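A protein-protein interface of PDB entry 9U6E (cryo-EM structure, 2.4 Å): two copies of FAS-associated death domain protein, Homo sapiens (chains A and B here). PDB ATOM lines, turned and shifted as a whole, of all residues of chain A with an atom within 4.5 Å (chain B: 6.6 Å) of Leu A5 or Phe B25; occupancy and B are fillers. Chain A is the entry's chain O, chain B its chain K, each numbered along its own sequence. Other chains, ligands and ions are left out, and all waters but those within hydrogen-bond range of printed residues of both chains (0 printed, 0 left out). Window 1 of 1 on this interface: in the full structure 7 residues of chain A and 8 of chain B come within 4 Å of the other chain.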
ATOM      1  N   ASP A   2      16.026  13.866 -24.043  1.00  0.00           N
ATOM      2  CA  ASP A   2      16.194  14.756 -25.182  1.00  0.00           C
ATOM      3  C   ASP A   2      16.865  14.023 -26.340  1.00  0.00           C
ATOM      4  O   ASP A   2      18.002  13.548 -26.189  1.00  0.00           O
ATOM      5  CB  ASP A   2      17.019  15.975 -24.776  1.00  0.00           C
ATOM      6  CG  ASP A   2      16.753  17.180 -25.654  1.00  0.00           C
ATOM      7  OD1 ASP A   2      16.515  16.998 -26.866  1.00  0.00           O
ATOM      8  OD2 ASP A   2      16.786  18.314 -25.133  1.00  0.00           O
ATOM      9  N   PRO A   3      16.209  13.906 -27.499  1.00  0.00           N
ATOM     10  CA  PRO A   3      16.863  13.253 -28.645  1.00  0.00           C
ATOM     11  C   PRO A   3      18.133  13.953 -29.098  1.00  0.00           C
ATOM     12  O   PRO A   3      19.079  13.285 -29.530  1.00  0.00           O
ATOM     13  CB  PRO A   3      15.775  13.288 -29.726  1.00  0.00           C
ATOM     14  CG  PRO A   3      14.495  13.372 -28.965  1.00  0.00           C
ATOM     15  CD  PRO A   3      14.802  14.235 -27.783  1.00  0.00           C
ATOM     16  N   PHE A   4      18.180  15.283 -29.018  1.00  0.00           N
ATOM     17  CA  PHE A   4      19.395  16.002 -29.386  1.00  0.00           C
ATOM     18  C   PHE A   4      20.550  15.640 -28.460  1.00  0.00           C
ATOM     19  O   PHE A   4      21.680  15.419 -28.916  1.00  0.00           O
ATOM     20  CB  PHE A   4      19.135  17.507 -29.367  1.00  0.00           C
ATOM     21  CG  PHE A   4      20.181  18.314 -30.075  1.00  0.00           C
ATOM     22  CD1 PHE A   4      20.516  18.041 -31.389  1.00  0.00           C
ATOM     23  CD2 PHE A   4      20.831  19.351 -29.427  1.00  0.00           C
ATOM     24  CE1 PHE A   4      21.479  18.783 -32.040  1.00  0.00           C
ATOM     25  CE2 PHE A   4      21.793  20.096 -30.074  1.00  0.00           C
ATOM     26  CZ  PHE A   4      22.116  19.812 -31.384  1.00  0.00           C
ATOM     27  N   LEU A   5      20.285  15.567 -27.153  1.00  0.00           N
ATOM     28  CA  LEU A   5      21.321  15.165 -26.210  1.00  0.00           C
ATOM     29  C   LEU A   5      21.753  13.722 -26.434  1.00  0.00           C
ATOM     30  O   LEU A   5      22.946  13.412 -26.331  1.00  0.00           O
ATOM     31  CB  LEU A   5      20.830  15.359 -24.776  1.00  0.00           C
ATOM     32  CG  LEU A   5      20.738  16.803 -24.278  1.00  0.00           C
ATOM     33  CD1 LEU A   5      20.552  16.839 -22.773  1.00  0.00           C
ATOM     34  CD2 LEU A   5      21.964  17.601 -24.687  1.00  0.00           C
ATOM     35  N   VAL A   6      20.806  12.832 -26.743  1.00  0.00           N
ATOM     36  CA  VAL A   6      21.168  11.449 -27.040  1.00  0.00           C
ATOM     37  C   VAL A   6      22.057  11.373 -28.276  1.00  0.00           C
ATOM     38  O   VAL A   6      23.053  10.638 -28.291  1.00  0.00           O
ATOM     39  CB  VAL A   6      19.901  10.587 -27.198  1.00  0.00           C
ATOM     40  CG1 VAL A   6      20.265   9.176 -27.628  1.00  0.00           C
ATOM     41  CG2 VAL A   6      19.122  10.557 -25.898  1.00  0.00           C
ATOM     42  N   LEU A   7      21.721  12.129 -29.325  1.00  0.00           N
ATOM     43  CA  LEU A   7      22.538  12.140 -30.534  1.00  0.00           C
ATOM     44  C   LEU A   7      23.936  12.675 -30.251  1.00  0.00           C
ATOM     45  O   LEU A   7      24.932  12.129 -30.740  1.00  0.00           O
ATOM     46  CB  LEU A   7      21.855  12.971 -31.618  1.00  0.00           C
ATOM     47  CG  LEU A   7      22.756  13.456 -32.756  1.00  0.00           C
ATOM     48  CD1 LEU A   7      22.977  12.350 -33.771  1.00  0.00           C
ATOM     49  CD2 LEU A   7      22.174  14.691 -33.420  1.00  0.00           C
ATOM     50  N   LEU A   8      24.031  13.754 -29.469  1.00  0.00           N
ATOM     51  CA  LEU A   8      25.341  14.310 -29.150  1.00  0.00           C
ATOM     52  C   LEU A   8      26.180  13.336 -28.332  1.00  0.00           C
ATOM     53  O   LEU A   8      27.387  13.206 -28.567  1.00  0.00           O
ATOM     54  CB  LEU A   8      25.187  15.636 -28.409  1.00  0.00           C
ATOM     55  CG  LEU A   8      24.625  16.800 -29.225  1.00  0.00           C
ATOM     56  CD1 LEU A   8      24.479  18.035 -28.358  1.00  0.00           C
ATOM     57  CD2 LEU A   8      25.504  17.086 -30.428  1.00  0.00           C
ATOM     58  N   HIS A   9      25.561  12.641 -27.375  1.00  0.00           N
ATOM     59  CA  HIS A   9      26.287  11.645 -26.594  1.00  0.00           C
ATOM     60  C   HIS A   9      26.763  10.496 -27.475  1.00  0.00           C
ATOM     61  O   HIS A   9      27.897  10.019 -27.329  1.00  0.00           O
ATOM     62  CB  HIS A   9      25.398  11.139 -25.457  1.00  0.00           C
ATOM     63  CG  HIS A   9      25.885   9.880 -24.813  1.00  0.00           C
ATOM     64  ND1 HIS A   9      26.867   9.872 -23.847  1.00  0.00           N
ATOM     65  CD2 HIS A   9      25.515   8.589 -24.985  1.00  0.00           C
ATOM     66  CE1 HIS A   9      27.088   8.629 -23.458  1.00  0.00           C
ATOM     67  NE2 HIS A   9      26.281   7.832 -24.134  1.00  0.00           N
ATOM     68  N   LEU A  43      31.721  15.608 -24.957  1.00  0.00           N
ATOM     69  CA  LEU A  43      30.567  16.129 -24.230  1.00  0.00           C
ATOM     70  C   LEU A  43      30.831  17.530 -23.696  1.00  0.00           C
ATOM     71  O   LEU A  43      29.946  18.393 -23.737  1.00  0.00           O
ATOM     72  CB  LEU A  43      30.200  15.181 -23.089  1.00  0.00           C
ATOM     73  CG  LEU A  43      29.737  13.779 -23.491  1.00  0.00           C
ATOM     74  CD1 LEU A  43      29.382  12.960 -22.267  1.00  0.00           C
ATOM     75  CD2 LEU A  43      28.564  13.850 -24.449  1.00  0.00           C
ATOM     76  N   SER A  47      28.722  20.814 -24.765  1.00  0.00           N
ATOM     77  CA  SER A  47      28.026  21.635 -23.778  1.00  0.00           C
ATOM     78  C   SER A  47      28.420  23.102 -23.905  1.00  0.00           C
ATOM     79  O   SER A  47      27.560  23.996 -23.879  1.00  0.00           O
ATOM     80  CB  SER A  47      28.322  21.123 -22.368  1.00  0.00           C
ATOM     81  OG  SER A  47      27.993  19.753 -22.244  1.00  0.00           O
ATOM     82  N   LEU A  50      26.771  24.519 -26.877  1.00  0.00           N
ATOM     83  CA  LEU A  50      25.345  24.712 -26.636  1.00  0.00           C
ATOM     84  C   LEU A  50      25.085  25.987 -25.848  1.00  0.00           C
ATOM     85  O   LEU A  50      24.114  26.702 -26.121  1.00  0.00           O
ATOM     86  CB  LEU A  50      24.764  23.510 -25.891  1.00  0.00           C
ATOM     87  CG  LEU A  50      24.420  22.250 -26.684  1.00  0.00           C
ATOM     88  CD1 LEU A  50      24.420  21.039 -25.769  1.00  0.00           C
ATOM     89  CD2 LEU A  50      23.077  22.400 -27.371  1.00  0.00           C
ATOM     90  N   LEU B  20      29.497   8.595 -14.647  1.00  0.00           N
ATOM     91  CA  LEU B  20      28.832   9.691 -13.950  1.00  0.00           C
ATOM     92  C   LEU B  20      28.850  10.968 -14.782  1.00  0.00           C
ATOM     93  O   LEU B  20      27.853  11.697 -14.840  1.00  0.00           O
ATOM     94  CB  LEU B  20      29.491   9.925 -12.593  1.00  0.00           C
ATOM     95  CG  LEU B  20      28.825  10.957 -11.681  1.00  0.00           C
ATOM     96  CD1 LEU B  20      27.428  10.507 -11.284  1.00  0.00           C
ATOM     97  CD2 LEU B  20      29.680  11.214 -10.454  1.00  0.00           C
ATOM     98  N   THR B  21      29.982  11.256 -15.430  1.00  0.00           N
ATOM     99  CA  THR B  21      30.057  12.415 -16.314  1.00  0.00           C
ATOM    100  C   THR B  21      29.094  12.272 -17.485  1.00  0.00           C
ATOM    101  O   THR B  21      28.457  13.248 -17.898  1.00  0.00           O
ATOM    102  CB  THR B  21      31.491  12.600 -16.812  1.00  0.00           C
ATOM    103  OG1 THR B  21      32.359  12.831 -15.696  1.00  0.00           O
ATOM    104  CG2 THR B  21      31.584  13.779 -17.765  1.00  0.00           C
ATOM    105  N   GLU B  22      28.976  11.063 -18.034  1.00  0.00           N
ATOM    106  CA  GLU B  22      28.001  10.818 -19.093  1.00  0.00           C
ATOM    107  C   GLU B  22      26.577  11.053 -18.602  1.00  0.00           C
ATOM    108  O   GLU B  22      25.760  11.647 -19.312  1.00  0.00           O
ATOM    109  CB  GLU B  22      28.150   9.392 -19.621  1.00  0.00           C
ATOM    110  CG  GLU B  22      29.291   9.200 -20.604  1.00  0.00           C
ATOM    111  CD  GLU B  22      29.606   7.737 -20.847  1.00  0.00           C
ATOM    112  OE1 GLU B  22      30.642   7.258 -20.342  1.00  0.00           O
ATOM    113  OE2 GLU B  22      28.817   7.061 -21.541  1.00  0.00           O
ATOM    114  N   LEU B  23      26.261  10.587 -17.391  1.00  0.00           N
ATOM    115  CA  LEU B  23      24.913  10.746 -16.855  1.00  0.00           C
ATOM    116  C   LEU B  23      24.582  12.204 -16.569  1.00  0.00           C
ATOM    117  O   LEU B  23      23.433  12.622 -16.750  1.00  0.00           O
ATOM    118  CB  LEU B  23      24.744   9.914 -15.584  1.00  0.00           C
ATOM    119  CG  LEU B  23      24.558   8.404 -15.736  1.00  0.00           C
ATOM    120  CD1 LEU B  23      24.501   7.740 -14.373  1.00  0.00           C
ATOM    121  CD2 LEU B  23      23.311   8.091 -16.537  1.00  0.00           C
ATOM    122  N   LYS B  24      25.561  12.988 -16.110  1.00  0.00           N
ATOM    123  CA  LYS B  24      25.304  14.402 -15.854  1.00  0.00           C
ATOM    124  C   LYS B  24      25.022  15.169 -17.139  1.00  0.00           C
ATOM    125  O   LYS B  24      24.221  16.109 -17.132  1.00  0.00           O
ATOM    126  CB  LYS B  24      26.481  15.026 -15.107  1.00  0.00           C
ATOM    127  CG  LYS B  24      26.604  14.575 -13.664  1.00  0.00           C
ATOM    128  CD  LYS B  24      27.960  14.928 -13.088  1.00  0.00           C
ATOM    129  CE  LYS B  24      28.207  16.422 -13.131  1.00  0.00           C
ATOM    130  NZ  LYS B  24      28.949  16.892 -11.933  1.00  0.00           N
ATOM    131  N   PHE B  25      25.668  14.792 -18.244  1.00  0.00           N
ATOM    132  CA  PHE B  25      25.407  15.443 -19.524  1.00  0.00           C
ATOM    133  C   PHE B  25      23.988  15.174 -20.012  1.00  0.00           C
ATOM    134  O   PHE B  25      23.330  16.076 -20.539  1.00  0.00           O
ATOM    135  CB  PHE B  25      26.428  14.982 -20.566  1.00  0.00           C
ATOM    136  CG  PHE B  25      26.148  15.482 -21.958  1.00  0.00           C
ATOM    137  CD1 PHE B  25      26.604  16.722 -22.367  1.00  0.00           C
ATOM    138  CD2 PHE B  25      25.440  14.705 -22.862  1.00  0.00           C
ATOM    139  CE1 PHE B  25      26.352  17.181 -23.644  1.00  0.00           C
ATOM    140  CE2 PHE B  25      25.185  15.162 -24.139  1.00  0.00           C
ATOM    141  CZ  PHE B  25      25.641  16.400 -24.530  1.00  0.00           C
ATOM    142  N   LEU B  26      23.503  13.941 -19.850  1.00  0.00           N
ATOM    143  CA  LEU B  26      22.173  13.588 -20.332  1.00  0.00           C
ATOM    144  C   LEU B  26      21.058  14.196 -19.495  1.00  0.00           C
ATOM    145  O   LEU B  26      19.895  14.126 -19.904  1.00  0.00           O
ATOM    146  CB  LEU B  26      22.017  12.067 -20.375  1.00  0.00           C
ATOM    147  CG  LEU B  26      22.897  11.319 -21.378  1.00  0.00           C
ATOM    148  CD1 LEU B  26      22.971   9.842 -21.032  1.00  0.00           C
ATOM    149  CD2 LEU B  26      22.388  11.513 -22.795  1.00  0.00           C
ATOM    150  N   CYS B  27      21.375  14.782 -18.342  1.00  0.00           N
ATOM    151  CA  CYS B  27      20.397  15.464 -17.504  1.00  0.00           C
ATOM    152  C   CYS B  27      20.578  16.979 -17.545  1.00  0.00           C
ATOM    153  O   CYS B  27      20.262  17.674 -16.578  1.00  0.00           O
ATOM    154  CB  CYS B  27      20.475  14.956 -16.066  1.00  0.00           C
ATOM    155  SG  CYS B  27      20.007  13.224 -15.855  1.00  0.00           S
ATOM    156  N   LEU B  28      21.094  17.498 -18.660  1.00  0.00           N
ATOM    157  CA  LEU B  28      21.330  18.934 -18.780  1.00  0.00           C
ATOM    158  C   LEU B  28      20.027  19.720 -18.739  1.00  0.00           C
ATOM    159  O   LEU B  28      19.949  20.773 -18.096  1.00  0.00           O
ATOM    160  CB  LEU B  28      22.088  19.232 -20.074  1.00  0.00           C
ATOM    161  CG  LEU B  28      23.611  19.321 -19.997  1.00  0.00           C
ATOM    162  CD1 LEU B  28      24.194  19.517 -21.385  1.00  0.00           C
ATOM    163  CD2 LEU B  28      24.041  20.443 -19.071  1.00  0.00           C
ATOM    164  N   GLY B  29      18.997  19.232 -19.423  1.00  0.00           N
ATOM    165  CA  GLY B  29      17.726  19.918 -19.479  1.00  0.00           C
ATOM    166  C   GLY B  29      16.805  19.683 -18.308  1.00  0.00           C
ATOM    167  O   GLY B  29      15.727  20.283 -18.250  1.00  0.00           O
ATOM    168  N   LEU B  36      23.916  20.785 -10.616  1.00  0.00           N
ATOM    169  CA  LEU B  36      24.701  19.696 -11.185  1.00  0.00           C
ATOM    170  C   LEU B  36      26.176  19.791 -10.820  1.00  0.00           C
ATOM    171  O   LEU B  36      26.879  18.777 -10.864  1.00  0.00           O
ATOM    172  CB  LEU B  36      24.541  19.672 -12.705  1.00  0.00           C
ATOM    173  CG  LEU B  36      23.421  18.784 -13.253  1.00  0.00           C
ATOM    174  CD1 LEU B  36      23.321  18.910 -14.763  1.00  0.00           C
ATOM    175  CD2 LEU B  36      23.630  17.338 -12.847  1.00  0.00           C
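No position is printed for both chains. Of the 7 pairs that touch across the chains among the printed residues, none has its exchanged pair printed and touching as well.
Hydrophobic or aromatic side chains of chain A within 4 Å of the printed part of chain B: Leu A5, Leu A8, His A9 and Leu A43.
The backbone carbonyl oxygen (O) of Leu A43 is in hydrogen-bond range of the side-chain hydroxyl (OG) of Ser A47.
Of the printed residues of chain B, Leu A5 touches Phe B25 and Leu B28. Of the printed residues of chain B, Leu A8 touches Phe B25 (3.98 Å). Of the printed residues of chain B, Leu A43 touches Phe B25. Of the printed residues of chain A, Glu B22 touches His A9 (3.0 Å). Of the printed residues of chain A, Phe B25 touches Leu A5 (3.6 Å), Leu A8 (3.98 Å), Leu A43 (3.6 Å) and Ser A47 (3.3 Å). Of the printed residues of chain A, Leu B28 touches Leu A5 (3.9 Å) and Ser A47 (3.9 Å). The nearest printed residue of chain B that does not touch Leu A5 is Leu B26 (4.003 Å).
Among the printed residues, merely in contact across the chains: Leu A5 with Phe B25 (3.6 Å), Leu A5 with Leu B28 (3.9 Å), Leu A8 with Phe B25 (3.98 Å), His A9 with Glu B22 (3.0 Å), Leu A43 with Phe B25 (3.6 Å), Ser A47 with Phe B25 (3.3 Å) and Ser A47 with Leu B28 (3.9 Å).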
